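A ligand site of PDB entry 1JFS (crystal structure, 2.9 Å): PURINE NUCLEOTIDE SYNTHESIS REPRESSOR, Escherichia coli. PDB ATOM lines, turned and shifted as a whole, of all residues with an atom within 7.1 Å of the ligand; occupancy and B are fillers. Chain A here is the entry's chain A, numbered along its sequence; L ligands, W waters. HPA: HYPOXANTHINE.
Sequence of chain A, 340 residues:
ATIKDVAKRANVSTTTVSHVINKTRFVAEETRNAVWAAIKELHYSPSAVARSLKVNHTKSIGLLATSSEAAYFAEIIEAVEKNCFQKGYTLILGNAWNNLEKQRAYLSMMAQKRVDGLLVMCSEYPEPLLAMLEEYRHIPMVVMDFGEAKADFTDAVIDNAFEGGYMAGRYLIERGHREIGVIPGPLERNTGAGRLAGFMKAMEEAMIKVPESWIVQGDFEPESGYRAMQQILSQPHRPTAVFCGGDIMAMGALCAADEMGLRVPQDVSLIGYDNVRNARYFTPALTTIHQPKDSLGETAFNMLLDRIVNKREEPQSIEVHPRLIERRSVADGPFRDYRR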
ATOM      1  N   THR A  66     -26.375  22.150  -5.925  1.00  0.00           N
ATOM      2  CA  THR A  66     -25.431  21.081  -6.090  1.00  0.00           C
ATOM      3  C   THR A  66     -26.263  19.814  -5.955  1.00  0.00           C
ATOM      4  O   THR A  66     -26.170  18.890  -6.755  1.00  0.00           O
ATOM      5  CB  THR A  66     -24.376  21.121  -4.968  1.00  0.00           C
ATOM      6  OG1 THR A  66     -23.365  22.083  -5.285  1.00  0.00           O
ATOM      7  CG2 THR A  66     -23.725  19.775  -4.832  1.00  0.00           C
ATOM      8  N   SER A  67     -27.102  19.804  -4.929  1.00  0.00           N
ATOM      9  CA  SER A  67     -27.953  18.672  -4.645  1.00  0.00           C
ATOM     10  C   SER A  67     -29.156  19.187  -3.825  1.00  0.00           C
ATOM     11  O   SER A  67     -29.047  20.097  -3.013  1.00  0.00           O
ATOM     12  CB  SER A  67     -27.122  17.606  -3.860  1.00  0.00           C
ATOM     13  OG  SER A  67     -27.908  16.740  -3.046  1.00  0.00           O
ATOM     14  N   ALA A  70     -29.644  16.409   0.450  1.00  0.00           N
ATOM     15  CA  ALA A  70     -28.845  16.666   1.639  1.00  0.00           C
ATOM     16  C   ALA A  70     -29.523  17.685   2.526  1.00  0.00           C
ATOM     17  O   ALA A  70     -29.847  18.797   2.082  1.00  0.00           O
ATOM     18  CB  ALA A  70     -27.490  17.172   1.213  1.00  0.00           C
ATOM     19  N   ALA A  71     -29.773  17.303   3.781  1.00  0.00           N
ATOM     20  CA  ALA A  71     -30.455  18.162   4.766  1.00  0.00           C
ATOM     21  C   ALA A  71     -30.056  19.630   4.733  1.00  0.00           C
ATOM     22  O   ALA A  71     -30.903  20.499   4.709  1.00  0.00           O
ATOM     23  CB  ALA A  71     -30.245  17.630   6.146  1.00  0.00           C
ATOM     24  N   TYR A  72     -28.756  19.869   4.757  1.00  0.00           N
ATOM     25  CA  TYR A  72     -28.196  21.194   4.744  1.00  0.00           C
ATOM     26  C   TYR A  72     -28.842  21.945   3.575  1.00  0.00           C
ATOM     27  O   TYR A  72     -29.615  22.902   3.726  1.00  0.00           O
ATOM     28  CB  TYR A  72     -26.684  21.048   4.538  1.00  0.00           C
ATOM     29  CG  TYR A  72     -26.014  22.352   4.465  1.00  0.00           C
ATOM     30  CD1 TYR A  72     -25.336  22.733   3.365  1.00  0.00           C
ATOM     31  CD2 TYR A  72     -26.098  23.225   5.511  1.00  0.00           C
ATOM     32  CE1 TYR A  72     -24.718  23.970   3.316  1.00  0.00           C
ATOM     33  CE2 TYR A  72     -25.496  24.456   5.476  1.00  0.00           C
ATOM     34  CZ  TYR A  72     -24.816  24.823   4.378  1.00  0.00           C
ATOM     35  OH  TYR A  72     -24.243  26.051   4.351  1.00  0.00           O
ATOM     36  N   PHE A  73     -28.557  21.437   2.409  1.00  0.00           N
ATOM     37  CA  PHE A  73     -29.042  21.965   1.198  1.00  0.00           C
ATOM     38  C   PHE A  73     -30.506  22.105   1.167  1.00  0.00           C
ATOM     39  O   PHE A  73     -31.040  23.161   0.853  1.00  0.00           O
ATOM     40  CB  PHE A  73     -28.668  21.008   0.130  1.00  0.00           C
ATOM     41  CG  PHE A  73     -27.238  21.105  -0.241  1.00  0.00           C
ATOM     42  CD1 PHE A  73     -26.553  20.003  -0.708  1.00  0.00           C
ATOM     43  CD2 PHE A  73     -26.585  22.317  -0.134  1.00  0.00           C
ATOM     44  CE1 PHE A  73     -25.224  20.112  -1.065  1.00  0.00           C
ATOM     45  CE2 PHE A  73     -25.268  22.440  -0.491  1.00  0.00           C
ATOM     46  CZ  PHE A  73     -24.580  21.332  -0.949  1.00  0.00           C
ATOM     47  N   SER A 123     -20.920  24.646  -4.450  1.00  0.00           N
ATOM     48  CA  SER A 123     -20.007  23.991  -3.526  1.00  0.00           C
ATOM     49  C   SER A 123     -18.616  24.204  -3.972  1.00  0.00           C
ATOM     50  O   SER A 123     -17.959  25.040  -3.417  1.00  0.00           O
ATOM     51  CB  SER A 123     -20.352  22.528  -3.411  1.00  0.00           C
ATOM     52  OG  SER A 123     -21.722  22.382  -3.064  1.00  0.00           O
ATOM     53  N   GLU A 124     -18.125  23.477  -4.974  1.00  0.00           N
ATOM     54  CA  GLU A 124     -16.747  23.726  -5.419  1.00  0.00           C
ATOM     55  C   GLU A 124     -16.735  24.702  -6.599  1.00  0.00           C
ATOM     56  O   GLU A 124     -17.676  24.691  -7.411  1.00  0.00           O
ATOM     57  CB  GLU A 124     -16.011  22.435  -5.749  1.00  0.00           C
ATOM     58  CG  GLU A 124     -16.408  21.325  -4.795  1.00  0.00           C
ATOM     59  CD  GLU A 124     -15.618  20.109  -5.024  1.00  0.00           C
ATOM     60  OE1 GLU A 124     -14.907  20.083  -6.068  1.00  0.00           O
ATOM     61  OE2 GLU A 124     -15.703  19.201  -4.167  1.00  0.00           O
ATOM     62  N   PRO A 186     -15.016  17.906   2.400  1.00  0.00           N
ATOM     63  CA  PRO A 186     -14.135  18.048   1.259  1.00  0.00           C
ATOM     64  C   PRO A 186     -13.464  19.409   1.208  1.00  0.00           C
ATOM     65  O   PRO A 186     -14.128  20.454   1.172  1.00  0.00           O
ATOM     66  CB  PRO A 186     -15.062  17.818   0.066  1.00  0.00           C
ATOM     67  CG  PRO A 186     -16.452  18.008   0.576  1.00  0.00           C
ATOM     68  CD  PRO A 186     -16.415  17.664   2.018  1.00  0.00           C
ATOM     69  N   ARG A 189     -14.108  22.721  -0.595  1.00  0.00           N
ATOM     70  CA  ARG A 189     -15.226  23.578  -0.177  1.00  0.00           C
ATOM     71  C   ARG A 189     -15.055  24.507   1.053  1.00  0.00           C
ATOM     72  O   ARG A 189     -14.272  24.245   1.979  1.00  0.00           O
ATOM     73  CB  ARG A 189     -16.527  22.782  -0.079  1.00  0.00           C
ATOM     74  CG  ARG A 189     -17.021  22.318  -1.419  1.00  0.00           C
ATOM     75  CD  ARG A 189     -17.197  20.811  -1.494  1.00  0.00           C
ATOM     76  NE  ARG A 189     -18.534  20.467  -1.072  1.00  0.00           N
ATOM     77  CZ  ARG A 189     -19.225  19.480  -1.600  1.00  0.00           C
ATOM     78  NH1 ARG A 189     -18.659  18.766  -2.556  1.00  0.00           N
ATOM     79  NH2 ARG A 189     -20.466  19.196  -1.196  1.00  0.00           N
ATOM     80  N   ASN A 190     -15.812  25.587   1.030  1.00  0.00           N
ATOM     81  CA  ASN A 190     -15.786  26.573   2.086  1.00  0.00           C
ATOM     82  C   ASN A 190     -16.121  25.918   3.383  1.00  0.00           C
ATOM     83  O   ASN A 190     -15.345  25.975   4.361  1.00  0.00           O
ATOM     84  CB  ASN A 190     -16.845  27.629   1.793  1.00  0.00           C
ATOM     85  CG  ASN A 190     -16.837  28.749   2.778  1.00  0.00           C
ATOM     86  OD1 ASN A 190     -15.764  29.273   3.145  1.00  0.00           O
ATOM     87  ND2 ASN A 190     -18.019  29.122   3.261  1.00  0.00           N
ATOM     88  N   THR A 191     -17.305  25.297   3.381  1.00  0.00           N
ATOM     89  CA  THR A 191     -17.825  24.588   4.522  1.00  0.00           C
ATOM     90  C   THR A 191     -16.832  23.455   4.898  1.00  0.00           C
ATOM     91  O   THR A 191     -16.875  22.941   6.006  1.00  0.00           O
ATOM     92  CB  THR A 191     -19.168  24.006   4.218  1.00  0.00           C
ATOM     93  OG1 THR A 191     -19.011  23.015   3.222  1.00  0.00           O
ATOM     94  CG2 THR A 191     -20.108  25.056   3.677  1.00  0.00           C
ATOM     95  N   GLY A 192     -15.941  23.091   3.967  1.00  0.00           N
ATOM     96  CA  GLY A 192     -14.946  22.061   4.223  1.00  0.00           C
ATOM     97  C   GLY A 192     -13.812  22.776   4.930  1.00  0.00           C
ATOM     98  O   GLY A 192     -13.812  22.953   6.143  1.00  0.00           O
ATOM     99  N   ARG A 195     -14.364  25.829   7.650  1.00  0.00           N
ATOM    100  CA  ARG A 195     -14.780  25.459   8.990  1.00  0.00           C
ATOM    101  C   ARG A 195     -13.549  24.874   9.722  1.00  0.00           C
ATOM    102  O   ARG A 195     -13.309  25.129  10.882  1.00  0.00           O
ATOM    103  CB  ARG A 195     -15.882  24.428   8.881  1.00  0.00           C
ATOM    104  CG  ARG A 195     -17.283  24.983   8.804  1.00  0.00           C
ATOM    105  CD  ARG A 195     -18.286  23.978   8.157  1.00  0.00           C
ATOM    106  NE  ARG A 195     -19.529  24.628   7.773  1.00  0.00           N
ATOM    107  CZ  ARG A 195     -20.703  24.016   7.773  1.00  0.00           C
ATOM    108  NH1 ARG A 195     -20.772  22.739   8.144  1.00  0.00           N
ATOM    109  NH2 ARG A 195     -21.806  24.676   7.410  1.00  0.00           N
ATOM    110  N   ASP A 219     -17.237  13.673   3.424  1.00  0.00           N
ATOM    111  CA  ASP A 219     -17.822  14.228   2.201  1.00  0.00           C
ATOM    112  C   ASP A 219     -19.206  14.752   2.476  1.00  0.00           C
ATOM    113  O   ASP A 219     -19.973  14.960   1.560  1.00  0.00           O
ATOM    114  CB  ASP A 219     -17.951  13.150   1.122  1.00  0.00           C
ATOM    115  CG  ASP A 219     -18.700  11.918   1.603  1.00  0.00           C
ATOM    116  OD1 ASP A 219     -18.567  10.866   0.956  1.00  0.00           O
ATOM    117  OD2 ASP A 219     -19.426  11.983   2.603  1.00  0.00           O
ATOM    118  N   PHE A 220     -19.514  14.937   3.743  1.00  0.00           N
ATOM    119  CA  PHE A 220     -20.830  15.428   4.183  1.00  0.00           C
ATOM    120  C   PHE A 220     -21.893  14.351   4.167  1.00  0.00           C
ATOM    121  O   PHE A 220     -23.097  14.629   4.356  1.00  0.00           O
ATOM    122  CB  PHE A 220     -21.274  16.649   3.370  1.00  0.00           C
ATOM    123  CG  PHE A 220     -20.497  17.879   3.668  1.00  0.00           C
ATOM    124  CD1 PHE A 220     -20.465  18.394   4.931  1.00  0.00           C
ATOM    125  CD2 PHE A 220     -19.784  18.504   2.681  1.00  0.00           C
ATOM    126  CE1 PHE A 220     -19.746  19.510   5.214  1.00  0.00           C
ATOM    127  CE2 PHE A 220     -19.059  19.625   2.952  1.00  0.00           C
ATOM    128  CZ  PHE A 220     -19.053  20.125   4.227  1.00  0.00           C
ATOM    129  N   GLU A 221     -21.466  13.123   3.937  1.00  0.00           N
ATOM    130  CA  GLU A 221     -22.394  11.994   3.908  1.00  0.00           C
ATOM    131  C   GLU A 221     -22.125  11.034   5.057  1.00  0.00           C
ATOM    132  O   GLU A 221     -20.980  10.608   5.331  1.00  0.00           O
ATOM    133  CB  GLU A 221     -22.451  11.284   2.545  1.00  0.00           C
ATOM    134  CG  GLU A 221     -22.805  12.223   1.385  1.00  0.00           C
ATOM    135  CD  GLU A 221     -24.256  12.132   0.930  1.00  0.00           C
ATOM    136  OE1 GLU A 221     -25.152  12.424   1.746  1.00  0.00           O
ATOM    137  OE2 GLU A 221     -24.480  11.805  -0.267  1.00  0.00           O
ATOM    138  N   GLY A 245     -17.175  18.073  10.852  1.00  0.00           N
ATOM    139  CA  GLY A 245     -17.388  19.136   9.856  1.00  0.00           C
ATOM    140  C   GLY A 245     -18.798  19.469   9.465  1.00  0.00           C
ATOM    141  O   GLY A 245     -19.025  20.522   8.868  1.00  0.00           O
ATOM    142  N   GLY A 246     -19.733  18.565   9.769  1.00  0.00           N
ATOM    143  CA  GLY A 246     -21.136  18.746   9.440  1.00  0.00           C
ATOM    144  C   GLY A 246     -22.005  17.703  10.172  1.00  0.00           C
ATOM    145  O   GLY A 246     -21.597  16.547  10.381  1.00  0.00           O
ATOM    146  N   ASP A 247     -23.211  18.112  10.576  1.00  0.00           N
ATOM    147  CA  ASP A 247     -24.136  17.250  11.266  1.00  0.00           C
ATOM    148  C   ASP A 247     -24.497  15.887  10.634  1.00  0.00           C
ATOM    149  O   ASP A 247     -24.555  14.880  11.337  1.00  0.00           O
ATOM    150  CB  ASP A 247     -25.403  18.008  11.538  1.00  0.00           C
ATOM    151  CG  ASP A 247     -25.193  19.182  12.480  1.00  0.00           C
ATOM    152  OD1 ASP A 247     -26.232  19.749  12.926  1.00  0.00           O
ATOM    153  OD2 ASP A 247     -24.028  19.521  12.753  1.00  0.00           O
ATOM    154  N   ILE A 248     -24.768  15.830   9.338  1.00  0.00           N
ATOM    155  CA  ILE A 248     -25.126  14.534   8.769  1.00  0.00           C
ATOM    156  C   ILE A 248     -23.974  13.578   8.936  1.00  0.00           C
ATOM    157  O   ILE A 248     -24.150  12.444   9.295  1.00  0.00           O
ATOM    158  CB  ILE A 248     -25.626  14.591   7.313  1.00  0.00           C
ATOM    159  CG1 ILE A 248     -26.825  15.494   7.226  1.00  0.00           C
ATOM    160  CG2 ILE A 248     -26.081  13.192   6.858  1.00  0.00           C
ATOM    161  CD1 ILE A 248     -27.843  14.937   8.144  1.00  0.00           C
ATOM    162  N   TYR A 273     -21.529  20.462  13.115  1.00  0.00           N
ATOM    163  CA  TYR A 273     -21.578  21.749  12.507  1.00  0.00           C
ATOM    164  C   TYR A 273     -22.638  21.728  11.412  1.00  0.00           C
ATOM    165  O   TYR A 273     -22.516  20.962  10.456  1.00  0.00           O
ATOM    166  CB  TYR A 273     -20.244  22.081  11.885  1.00  0.00           C
ATOM    167  CG  TYR A 273     -20.077  23.564  11.584  1.00  0.00           C
ATOM    168  CD1 TYR A 273     -18.882  24.222  11.860  1.00  0.00           C
ATOM    169  CD2 TYR A 273     -21.136  24.323  11.025  1.00  0.00           C
ATOM    170  CE1 TYR A 273     -18.737  25.563  11.588  1.00  0.00           C
ATOM    171  CE2 TYR A 273     -20.992  25.663  10.753  1.00  0.00           C
ATOM    172  CZ  TYR A 273     -19.801  26.280  11.042  1.00  0.00           C
ATOM    173  OH  TYR A 273     -19.673  27.591  10.782  1.00  0.00           O
ATOM    174  N   ASP A 274     -23.638  22.610  11.589  1.00  0.00           N
ATOM    175  CA  ASP A 274     -24.783  22.848  10.702  1.00  0.00           C
ATOM    176  C   ASP A 274     -26.094  23.186  11.424  1.00  0.00           C
ATOM    177  O   ASP A 274     -26.809  24.113  11.100  1.00  0.00           O
ATOM    178  CB  ASP A 274     -25.052  21.691   9.741  1.00  0.00           C
ATOM    179  CG  ASP A 274     -24.250  21.787   8.452  1.00  0.00           C
ATOM    180  OD1 ASP A 274     -24.430  20.897   7.577  1.00  0.00           O
ATOM    181  OD2 ASP A 274     -23.460  22.754   8.281  1.00  0.00           O
ATOM    182  N   VAL A 276     -28.993  21.259  11.741  1.00  0.00           N
ATOM    183  CA  VAL A 276     -30.096  21.010  10.847  1.00  0.00           C
ATOM    184  C   VAL A 276     -31.302  20.600  11.721  1.00  0.00           C
ATOM    185  O   VAL A 276     -31.139  20.013  12.804  1.00  0.00           O
ATOM    186  CB  VAL A 276     -29.759  19.832   9.886  1.00  0.00           C
ATOM    187  CG1 VAL A 276     -28.530  20.116   9.025  1.00  0.00           C
ATOM    188  CG2 VAL A 276     -29.516  18.573  10.716  1.00  0.00           C
ATOM    189  N   GLN A 291     -25.722  27.107  11.647  1.00  0.00           N
ATOM    190  CA  GLN A 291     -25.581  28.036  10.507  1.00  0.00           C
ATOM    191  C   GLN A 291     -26.951  28.532  10.189  1.00  0.00           C
ATOM    192  O   GLN A 291     -27.868  27.737   9.984  1.00  0.00           O
ATOM    193  CB  GLN A 291     -25.104  27.339   9.236  1.00  0.00           C
ATOM    194  CG  GLN A 291     -25.020  28.300   8.049  1.00  0.00           C
ATOM    195  CD  GLN A 291     -23.530  28.482   7.503  1.00  0.00           C
ATOM    196  OE1 GLN A 291     -23.258  28.141   6.370  1.00  0.00           O
ATOM    197  NE2 GLN A 291     -22.597  29.010   8.342  1.00  0.00           N
HETATM  198  N1  HPA L   1     -22.793  19.536   1.379  1.00  0.00           N
HETATM  199  C2  HPA L   1     -23.702  18.979   2.240  1.00  0.00           C
HETATM  200  N3  HPA L   1     -23.944  19.413   3.468  1.00  0.00           N
HETATM  201  C4  HPA L   1     -23.171  20.479   3.788  1.00  0.00           C
HETATM  202  C5  HPA L   1     -22.236  21.107   2.999  1.00  0.00           C
HETATM  203  C6  HPA L   1     -21.995  20.631   1.685  1.00  0.00           C
HETATM  204  O6  HPA L   1     -21.199  21.065   0.834  1.00  0.00           O
HETATM  205  N7  HPA L   1     -21.648  22.157   3.696  1.00  0.00           N
HETATM  206  C8  HPA L   1     -22.253  22.152   4.857  1.00  0.00           C
HETATM  207  N9  HPA L   1     -23.202  21.181   4.979  1.00  0.00           N
HETATM  208  O   HOH W   1     -22.682  17.182  -0.616  1.00  0.00           O
HETATM  209  O   HOH W   2     -26.691  18.155   4.765  1.00  0.00           O
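N7 of the ligand is in hydrogen-bond range of OG1 of Thr 191, 2.8 Å away. O6 of the ligand sits at hydrogen-bond distance from NH2 of Arg 189, 2.9 Å away. The side-chain carboxylate of Asp 274 sits at hydrogen-bond distance from a nitrogen (N9) of the ligand (2.9 Å).
Water W1 lies within hydrogen-bond range of the guanidinium group (NH2) of Arg 189 (3.1 Å) and a nitrogen (N1) of the ligand (3.1 Å). Water W2 lies within hydrogen-bond range of the backbone NH of Tyr 72, a nitrogen (N3) of the ligand and the backbone NH of Ala 71.
Tyr 72 touches the ligand. Phe 73 touches the ligand. NH2 of Arg 195 touches C8 of the ligand, at 3.6 Å. CD2 of Phe 220 touches C6 of the ligand, 3.2 Å away. Of the 25 residues printed, 7 come within 4 Å of the ligand. The nearest printed residue that does not touch the ligand is Ser 123 (4.1 Å).
N of Arg 195 is in hydrogen-bond range of O of Asn 190 (3.4 Å). The backbone carbonyl oxygen (O) of Asp 274 lies within hydrogen-bond range of the backbone NH (N) of Gln 291 (3.2 Å). N of Asp 274 is in hydrogen-bond range of OD2 of Asp 247 (3.3 Å). The backbone carbonyl oxygen of Tyr 273 sits close to the guanidinium group of Arg 195 (3.4 Å). NH2 of Arg 195 is in salt-bridge range of OD2 of Asp 274, at 2.7 Å. NH1 of Arg 189 lies within salt-bridge range of OE2 of Glu 124 (3.4 Å). The side-chain hydroxyl of Tyr 72 is in hydrogen-bond range of the side-chain amide oxygen of Gln 291, at 3.1 Å. The backbone carbonyl oxygen (O) of Gly 245 is in hydrogen-bond range of the guanidinium group (NH1) of Arg 195, at 2.9 Å.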
